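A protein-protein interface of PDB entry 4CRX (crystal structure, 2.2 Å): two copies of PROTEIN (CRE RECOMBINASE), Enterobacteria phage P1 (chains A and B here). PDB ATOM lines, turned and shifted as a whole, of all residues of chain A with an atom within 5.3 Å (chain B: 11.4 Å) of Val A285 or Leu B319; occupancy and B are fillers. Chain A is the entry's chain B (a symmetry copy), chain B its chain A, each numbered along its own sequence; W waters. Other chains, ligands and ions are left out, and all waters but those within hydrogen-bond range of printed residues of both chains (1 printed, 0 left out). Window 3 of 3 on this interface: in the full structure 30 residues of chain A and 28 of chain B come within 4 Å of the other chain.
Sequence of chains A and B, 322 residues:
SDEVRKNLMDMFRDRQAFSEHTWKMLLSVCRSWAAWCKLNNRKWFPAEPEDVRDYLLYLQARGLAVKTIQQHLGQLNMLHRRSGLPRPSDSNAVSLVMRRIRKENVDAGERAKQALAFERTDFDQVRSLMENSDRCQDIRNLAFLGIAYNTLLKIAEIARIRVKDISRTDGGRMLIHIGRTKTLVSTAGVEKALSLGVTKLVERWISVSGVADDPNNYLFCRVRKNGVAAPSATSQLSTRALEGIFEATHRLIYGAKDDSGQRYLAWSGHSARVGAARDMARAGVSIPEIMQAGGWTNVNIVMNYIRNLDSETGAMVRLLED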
ATOM      1  N   ARG A 120      20.850 -28.803  36.594  1.00  0.00           N
ATOM      2  CA  ARG A 120      20.634 -30.016  35.815  1.00  0.00           C
ATOM      3  C   ARG A 120      20.682 -31.293  36.652  1.00  0.00           C
ATOM      4  O   ARG A 120      19.793 -32.138  36.556  1.00  0.00           O
ATOM      5  CB  ARG A 120      21.687 -30.080  34.701  1.00  0.00           C
ATOM      6  CG  ARG A 120      21.623 -31.301  33.801  1.00  0.00           C
ATOM      7  CD  ARG A 120      20.247 -31.467  33.194  1.00  0.00           C
ATOM      8  NE  ARG A 120      20.201 -32.537  32.201  1.00  0.00           N
ATOM      9  CZ  ARG A 120      20.709 -32.447  30.975  1.00  0.00           C
ATOM     10  NH1 ARG A 120      21.306 -31.331  30.579  1.00  0.00           N
ATOM     11  NH2 ARG A 120      20.602 -33.469  30.137  1.00  0.00           N
ATOM     12  N   ASP A 279      24.432 -23.277  34.548  1.00  0.00           N
ATOM     13  CA  ASP A 279      24.698 -24.557  33.887  1.00  0.00           C
ATOM     14  C   ASP A 279      25.166 -24.198  32.469  1.00  0.00           C
ATOM     15  O   ASP A 279      26.057 -24.841  31.903  1.00  0.00           O
ATOM     16  CB  ASP A 279      23.425 -25.412  33.831  1.00  0.00           C
ATOM     17  CG  ASP A 279      23.225 -26.255  35.081  1.00  0.00           C
ATOM     18  OD1 ASP A 279      24.187 -26.422  35.865  1.00  0.00           O
ATOM     19  OD2 ASP A 279      22.098 -26.756  35.290  1.00  0.00           O
ATOM     20  N   MET A 280      24.544 -23.157  31.914  1.00  0.00           N
ATOM     21  CA  MET A 280      24.871 -22.629  30.590  1.00  0.00           C
ATOM     22  C   MET A 280      26.248 -21.969  30.679  1.00  0.00           C
ATOM     23  O   MET A 280      27.111 -22.193  29.829  1.00  0.00           O
ATOM     24  CB  MET A 280      23.838 -21.574  30.180  1.00  0.00           C
ATOM     25  CG  MET A 280      22.579 -22.126  29.529  1.00  0.00           C
ATOM     26  SD  MET A 280      21.283 -20.859  29.403  1.00  0.00           S
ATOM     27  CE  MET A 280      21.002 -20.691  27.622  1.00  0.00           C
ATOM     28  N   ALA A 281      26.427 -21.141  31.710  1.00  0.00           N
ATOM     29  CA  ALA A 281      27.690 -20.444  31.962  1.00  0.00           C
ATOM     30  C   ALA A 281      28.823 -21.455  31.889  1.00  0.00           C
ATOM     31  O   ALA A 281      29.850 -21.222  31.260  1.00  0.00           O
ATOM     32  CB  ALA A 281      27.670 -19.783  33.357  1.00  0.00           C
ATOM     33  N   ALA A 283      28.657 -24.389  30.529  1.00  0.00           N
ATOM     34  CA  ALA A 283      28.600 -25.192  29.331  1.00  0.00           C
ATOM     35  C   ALA A 283      29.331 -24.520  28.215  1.00  0.00           C
ATOM     36  O   ALA A 283      29.654 -25.136  27.195  1.00  0.00           O
ATOM     37  CB  ALA A 283      27.161 -25.416  28.960  1.00  0.00           C
ATOM     38  N   GLY A 284      29.578 -23.239  28.439  1.00  0.00           N
ATOM     39  CA  GLY A 284      30.273 -22.427  27.474  1.00  0.00           C
ATOM     40  C   GLY A 284      29.303 -21.671  26.595  1.00  0.00           C
ATOM     41  O   GLY A 284      29.727 -21.006  25.657  1.00  0.00           O
ATOM     42  N   VAL A 285      28.004 -21.776  26.869  1.00  0.00           N
ATOM     43  CA  VAL A 285      27.039 -21.045  26.057  1.00  0.00           C
ATOM     44  C   VAL A 285      27.494 -19.586  26.074  1.00  0.00           C
ATOM     45  O   VAL A 285      28.102 -19.130  27.044  1.00  0.00           O
ATOM     46  CB  VAL A 285      25.597 -21.165  26.617  1.00  0.00           C
ATOM     47  CG1 VAL A 285      24.620 -20.426  25.719  1.00  0.00           C
ATOM     48  CG2 VAL A 285      25.188 -22.622  26.698  1.00  0.00           C
ATOM     49  N   SER A 286      27.216 -18.863  24.996  1.00  0.00           N
ATOM     50  CA  SER A 286      27.620 -17.466  24.878  1.00  0.00           C
ATOM     51  C   SER A 286      26.765 -16.503  25.693  1.00  0.00           C
ATOM     52  O   SER A 286      25.559 -16.699  25.836  1.00  0.00           O
ATOM     53  CB  SER A 286      27.575 -17.045  23.411  1.00  0.00           C
ATOM     54  OG  SER A 286      26.274 -17.233  22.886  1.00  0.00           O
ATOM     55  N   ILE A 287      27.404 -15.455  26.210  1.00  0.00           N
ATOM     56  CA  ILE A 287      26.725 -14.434  27.003  1.00  0.00           C
ATOM     57  C   ILE A 287      25.420 -13.984  26.352  1.00  0.00           C
ATOM     58  O   ILE A 287      24.409 -13.823  27.031  1.00  0.00           O
ATOM     59  CB  ILE A 287      27.632 -13.192  27.213  1.00  0.00           C
ATOM     60  CG1 ILE A 287      28.461 -13.357  28.487  1.00  0.00           C
ATOM     61  CG2 ILE A 287      26.784 -11.931  27.317  1.00  0.00           C
ATOM     62  CD1 ILE A 287      28.903 -14.781  28.764  1.00  0.00           C
ATOM     63  N   GLU A 289      23.450 -15.620  24.204  1.00  0.00           N
ATOM     64  CA  GLU A 289      22.473 -16.710  24.193  1.00  0.00           C
ATOM     65  C   GLU A 289      21.874 -16.892  25.584  1.00  0.00           C
ATOM     66  O   GLU A 289      20.680 -17.161  25.735  1.00  0.00           O
ATOM     67  CB  GLU A 289      23.142 -18.012  23.755  1.00  0.00           C
ATOM     68  CG  GLU A 289      22.922 -18.364  22.302  1.00  0.00           C
ATOM     69  CD  GLU A 289      23.430 -19.745  21.964  1.00  0.00           C
ATOM     70  OE1 GLU A 289      24.623 -20.020  22.216  1.00  0.00           O
ATOM     71  OE2 GLU A 289      22.635 -20.554  21.446  1.00  0.00           O
ATOM     72  N   ILE A 290      22.728 -16.762  26.592  1.00  0.00           N
ATOM     73  CA  ILE A 290      22.312 -16.876  27.981  1.00  0.00           C
ATOM     74  C   ILE A 290      21.299 -15.770  28.231  1.00  0.00           C
ATOM     75  O   ILE A 290      20.171 -16.023  28.650  1.00  0.00           O
ATOM     76  CB  ILE A 290      23.504 -16.676  28.935  1.00  0.00           C
ATOM     77  CG1 ILE A 290      24.521 -17.804  28.737  1.00  0.00           C
ATOM     78  CG2 ILE A 290      23.018 -16.629  30.375  1.00  0.00           C
ATOM     79  CD1 ILE A 290      25.561 -17.890  29.833  1.00  0.00           C
ATOM     80  N   ASP B 310      12.367 -25.022  14.604  1.00  0.00           N
ATOM     81  CA  ASP B 310      13.192 -25.856  15.469  1.00  0.00           C
ATOM     82  C   ASP B 310      14.628 -25.354  15.562  1.00  0.00           C
ATOM     83  O   ASP B 310      15.318 -25.614  16.546  1.00  0.00           O
ATOM     84  CB  ASP B 310      13.196 -27.300  14.965  1.00  0.00           C
ATOM     85  CG  ASP B 310      11.995 -28.085  15.447  1.00  0.00           C
ATOM     86  OD1 ASP B 310      11.919 -28.370  16.660  1.00  0.00           O
ATOM     87  OD2 ASP B 310      11.127 -28.415  14.613  1.00  0.00           O
ATOM     88  N   THR B 313      15.220 -22.899  18.727  1.00  0.00           N
ATOM     89  CA  THR B 313      14.790 -23.310  20.062  1.00  0.00           C
ATOM     90  C   THR B 313      15.694 -22.912  21.234  1.00  0.00           C
ATOM     91  O   THR B 313      15.271 -23.000  22.383  1.00  0.00           O
ATOM     92  CB  THR B 313      14.531 -24.833  20.127  1.00  0.00           C
ATOM     93  OG1 THR B 313      15.668 -25.542  19.626  1.00  0.00           O
ATOM     94  CG2 THR B 313      13.307 -25.195  19.299  1.00  0.00           C
ATOM     95  N   GLY B 314      16.928 -22.493  20.961  1.00  0.00           N
ATOM     96  CA  GLY B 314      17.807 -22.053  22.037  1.00  0.00           C
ATOM     97  C   GLY B 314      18.766 -23.017  22.720  1.00  0.00           C
ATOM     98  O   GLY B 314      18.657 -24.235  22.594  1.00  0.00           O
ATOM     99  N   ALA B 315      19.698 -22.443  23.478  1.00  0.00           N
ATOM    100  CA  ALA B 315      20.719 -23.198  24.197  1.00  0.00           C
ATOM    101  C   ALA B 315      20.217 -24.204  25.241  1.00  0.00           C
ATOM    102  O   ALA B 315      20.813 -25.269  25.393  1.00  0.00           O
ATOM    103  CB  ALA B 315      21.706 -22.229  24.843  1.00  0.00           C
ATOM    104  N   MET B 316      19.141 -23.878  25.961  1.00  0.00           N
ATOM    105  CA  MET B 316      18.604 -24.788  26.983  1.00  0.00           C
ATOM    106  C   MET B 316      18.088 -26.089  26.362  1.00  0.00           C
ATOM    107  O   MET B 316      18.380 -27.180  26.856  1.00  0.00           O
ATOM    108  CB  MET B 316      17.474 -24.119  27.781  1.00  0.00           C
ATOM    109  CG  MET B 316      17.909 -23.208  28.952  1.00  0.00           C
ATOM    110  SD  MET B 316      19.395 -23.659  29.919  1.00  0.00           S
ATOM    111  CE  MET B 316      18.841 -25.118  30.806  1.00  0.00           C
ATOM    112  N   VAL B 317      17.311 -25.981  25.289  1.00  0.00           N
ATOM    113  CA  VAL B 317      16.802 -27.176  24.626  1.00  0.00           C
ATOM    114  C   VAL B 317      18.024 -27.975  24.184  1.00  0.00           C
ATOM    115  O   VAL B 317      18.027 -29.203  24.223  1.00  0.00           O
ATOM    116  CB  VAL B 317      15.966 -26.825  23.378  1.00  0.00           C
ATOM    117  CG1 VAL B 317      15.795 -28.057  22.509  1.00  0.00           C
ATOM    118  CG2 VAL B 317      14.613 -26.279  23.797  1.00  0.00           C
ATOM    119  N   ARG B 318      19.061 -27.251  23.776  1.00  0.00           N
ATOM    120  CA  ARG B 318      20.318 -27.835  23.315  1.00  0.00           C
ATOM    121  C   ARG B 318      21.088 -28.594  24.405  1.00  0.00           C
ATOM    122  O   ARG B 318      21.648 -29.661  24.148  1.00  0.00           O
ATOM    123  CB  ARG B 318      21.204 -26.730  22.737  1.00  0.00           C
ATOM    124  CG  ARG B 318      22.146 -27.188  21.642  1.00  0.00           C
ATOM    125  CD  ARG B 318      22.638 -26.014  20.818  1.00  0.00           C
ATOM    126  NE  ARG B 318      23.657 -25.241  21.521  1.00  0.00           N
ATOM    127  CZ  ARG B 318      23.590 -23.930  21.717  1.00  0.00           C
ATOM    128  NH1 ARG B 318      22.552 -23.246  21.258  1.00  0.00           N
ATOM    129  NH2 ARG B 318      24.562 -23.300  22.363  1.00  0.00           N
ATOM    130  N   LEU B 319      21.123 -28.031  25.610  1.00  0.00           N
ATOM    131  CA  LEU B 319      21.815 -28.639  26.751  1.00  0.00           C
ATOM    132  C   LEU B 319      21.010 -29.815  27.296  1.00  0.00           C
ATOM    133  O   LEU B 319      21.562 -30.832  27.722  1.00  0.00           O
ATOM    134  CB  LEU B 319      21.985 -27.606  27.874  1.00  0.00           C
ATOM    135  CG  LEU B 319      23.228 -26.714  27.935  1.00  0.00           C
ATOM    136  CD1 LEU B 319      23.433 -26.007  26.605  1.00  0.00           C
ATOM    137  CD2 LEU B 319      23.060 -25.695  29.059  1.00  0.00           C
ATOM    138  N   LEU B 320      19.694 -29.659  27.285  1.00  0.00           N
ATOM    139  CA  LEU B 320      18.811 -30.691  27.795  1.00  0.00           C
ATOM    140  C   LEU B 320      18.840 -31.963  26.963  1.00  0.00           C
ATOM    141  O   LEU B 320      18.773 -33.064  27.506  1.00  0.00           O
ATOM    142  CB  LEU B 320      17.387 -30.149  27.887  1.00  0.00           C
ATOM    143  CG  LEU B 320      17.173 -29.326  29.159  1.00  0.00           C
ATOM    144  CD1 LEU B 320      15.809 -28.676  29.141  1.00  0.00           C
ATOM    145  CD2 LEU B 320      17.319 -30.231  30.364  1.00  0.00           C
ATOM    146  N   GLU B 321      18.952 -31.821  25.649  1.00  0.00           N
ATOM    147  CA  GLU B 321      18.983 -32.990  24.775  1.00  0.00           C
ATOM    148  C   GLU B 321      20.404 -33.539  24.632  1.00  0.00           C
ATOM    149  O   GLU B 321      20.729 -34.230  23.673  1.00  0.00           O
ATOM    150  CB  GLU B 321      18.396 -32.618  23.411  1.00  0.00           C
ATOM    151  CG  GLU B 321      16.991 -32.035  23.528  1.00  0.00           C
ATOM    152  CD  GLU B 321      16.219 -32.050  22.226  1.00  0.00           C
ATOM    153  OE1 GLU B 321      16.843 -32.235  21.162  1.00  0.00           O
ATOM    154  OE2 GLU B 321      14.983 -31.871  22.271  1.00  0.00           O
ATOM    155  N   ASP B 322      21.226 -33.247  25.634  1.00  0.00           N
ATOM    156  CA  ASP B 322      22.639 -33.644  25.714  1.00  0.00           C
ATOM    157  C   ASP B 322      23.590 -33.837  24.471  1.00  0.00           C
ATOM    158  O   ASP B 322      24.453 -33.411  23.732  1.00  0.00           O
ATOM    159  CB  ASP B 322      22.751 -34.922  26.532  1.00  0.00           C
ATOM    160  CG  ASP B 322      23.091 -34.655  27.973  1.00  0.00           C
ATOM    161  OD1 ASP B 322      23.944 -33.782  28.216  1.00  0.00           O
ATOM    162  OD2 ASP B 322      22.490 -35.274  28.871  1.00  0.00           O
ATOM    163  OXT ASP B 322      24.297 -34.709  24.849  1.00  0.00           O
HETATM  164  O   HOH W   1      19.715 -19.454  23.328  1.00  0.00           O
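The side-chain carboxylate (OE1) of Glu A289 is in hydrogen-bond range of the side-chain hydroxyl (OG) of Ser A286, at 3.3 Å.
The side-chain carboxylate (OD2) of Asp A279 sits at hydrogen-bond distance from the backbone NH (N) of Arg A120 (2.7 Å).
N of Val A285 sits at hydrogen-bond distance from O of Met A280.
No residue of chain B comes within 4 Å of Asp A279.
Ala A281 touches none of the printed residues of chain B.
Val A285 touches just these residues of chain B: Ala B315 (3.5 Å) and Leu B319 (3.8 Å).
No residue of chain B comes within 4 Å of Ile A287.
Glu A289 touches just these residues of chain B: Ala B315 (3.9 Å) and Arg B318 (2.7 Å).
Asp B310 touches none of the printed residues of chain A.
Thr B313 touches none of the printed residues of chain A.
Printed residues of chain A within 4 Å of Ala B315: Met A280 (3.3 Å), Val A285 (3.5 Å) and Glu A289 (3.9 Å).
Printed residues of chain A within 4 Å of Met B316: Met A280 (3.4 Å).
Of the printed residues of chain A, Arg B318 touches Glu A289 (2.7 Å).
Of chain A, only Arg A120, Met A280 and Val A285 come within 4 Å of Leu B319.
Of the printed residues of chain A, Asp B322 touches Arg A120 (2.9 Å).
The nearest residue of chain B that does not touch Val A285 is Arg B318 (4.4 Å).
The nearest residue of chain A that does not touch Leu B319 is Ala A283 (4.1 Å).
The nearest printed residue of chain A that does not touch Arg B318 is Val A285 (4.4 Å).
Among the printed residues, merely in contact across the chains: Met A280 with Ala B315 (3.3 Å), Met A280 with Leu B319 (3.6 Å), Val A285 with Ala B315 (3.5 Å), Val A285 with Leu B319 (3.8 Å) and Glu A289 with Ala B315 (3.9 Å).
NH2 of Arg A120 lies within hydrogen-bond range of O of Leu B320.
The guanidinium group of Arg A120 is in hydrogen-bond range of the backbone carbonyl oxygen of Leu B319, 2.9 Å away.
The side-chain carboxylate (OE2) of Glu A289 is in salt-bridge range of the guanidinium group (NH1) of Arg B318, at 2.7 Å.
The guanidinium group (NH2) of Arg A120 lies within salt-bridge range of the side-chain carboxylate (OD2) of Asp B322 (2.9 Å).
The side-chain sulfur of Met A280 sits close to the side-chain sulfur of Met B316, at 3.4 Å.
Of the 11 printed residues of chain A, 4 touch a printed residue of chain B.
Hydrophobic or aromatic side chains of chain A within 4 Å of the printed part of chain B: Met A280 and Val A285.
Among the printed residues, 10 pairs touch across the chains.
Water W1 lies within hydrogen-bond range of the backbone NH of Ala B315 (3.0 Å) and the backbone carbonyl oxygen of Glu A289 (3.5 Å).
No position is printed for both chains.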
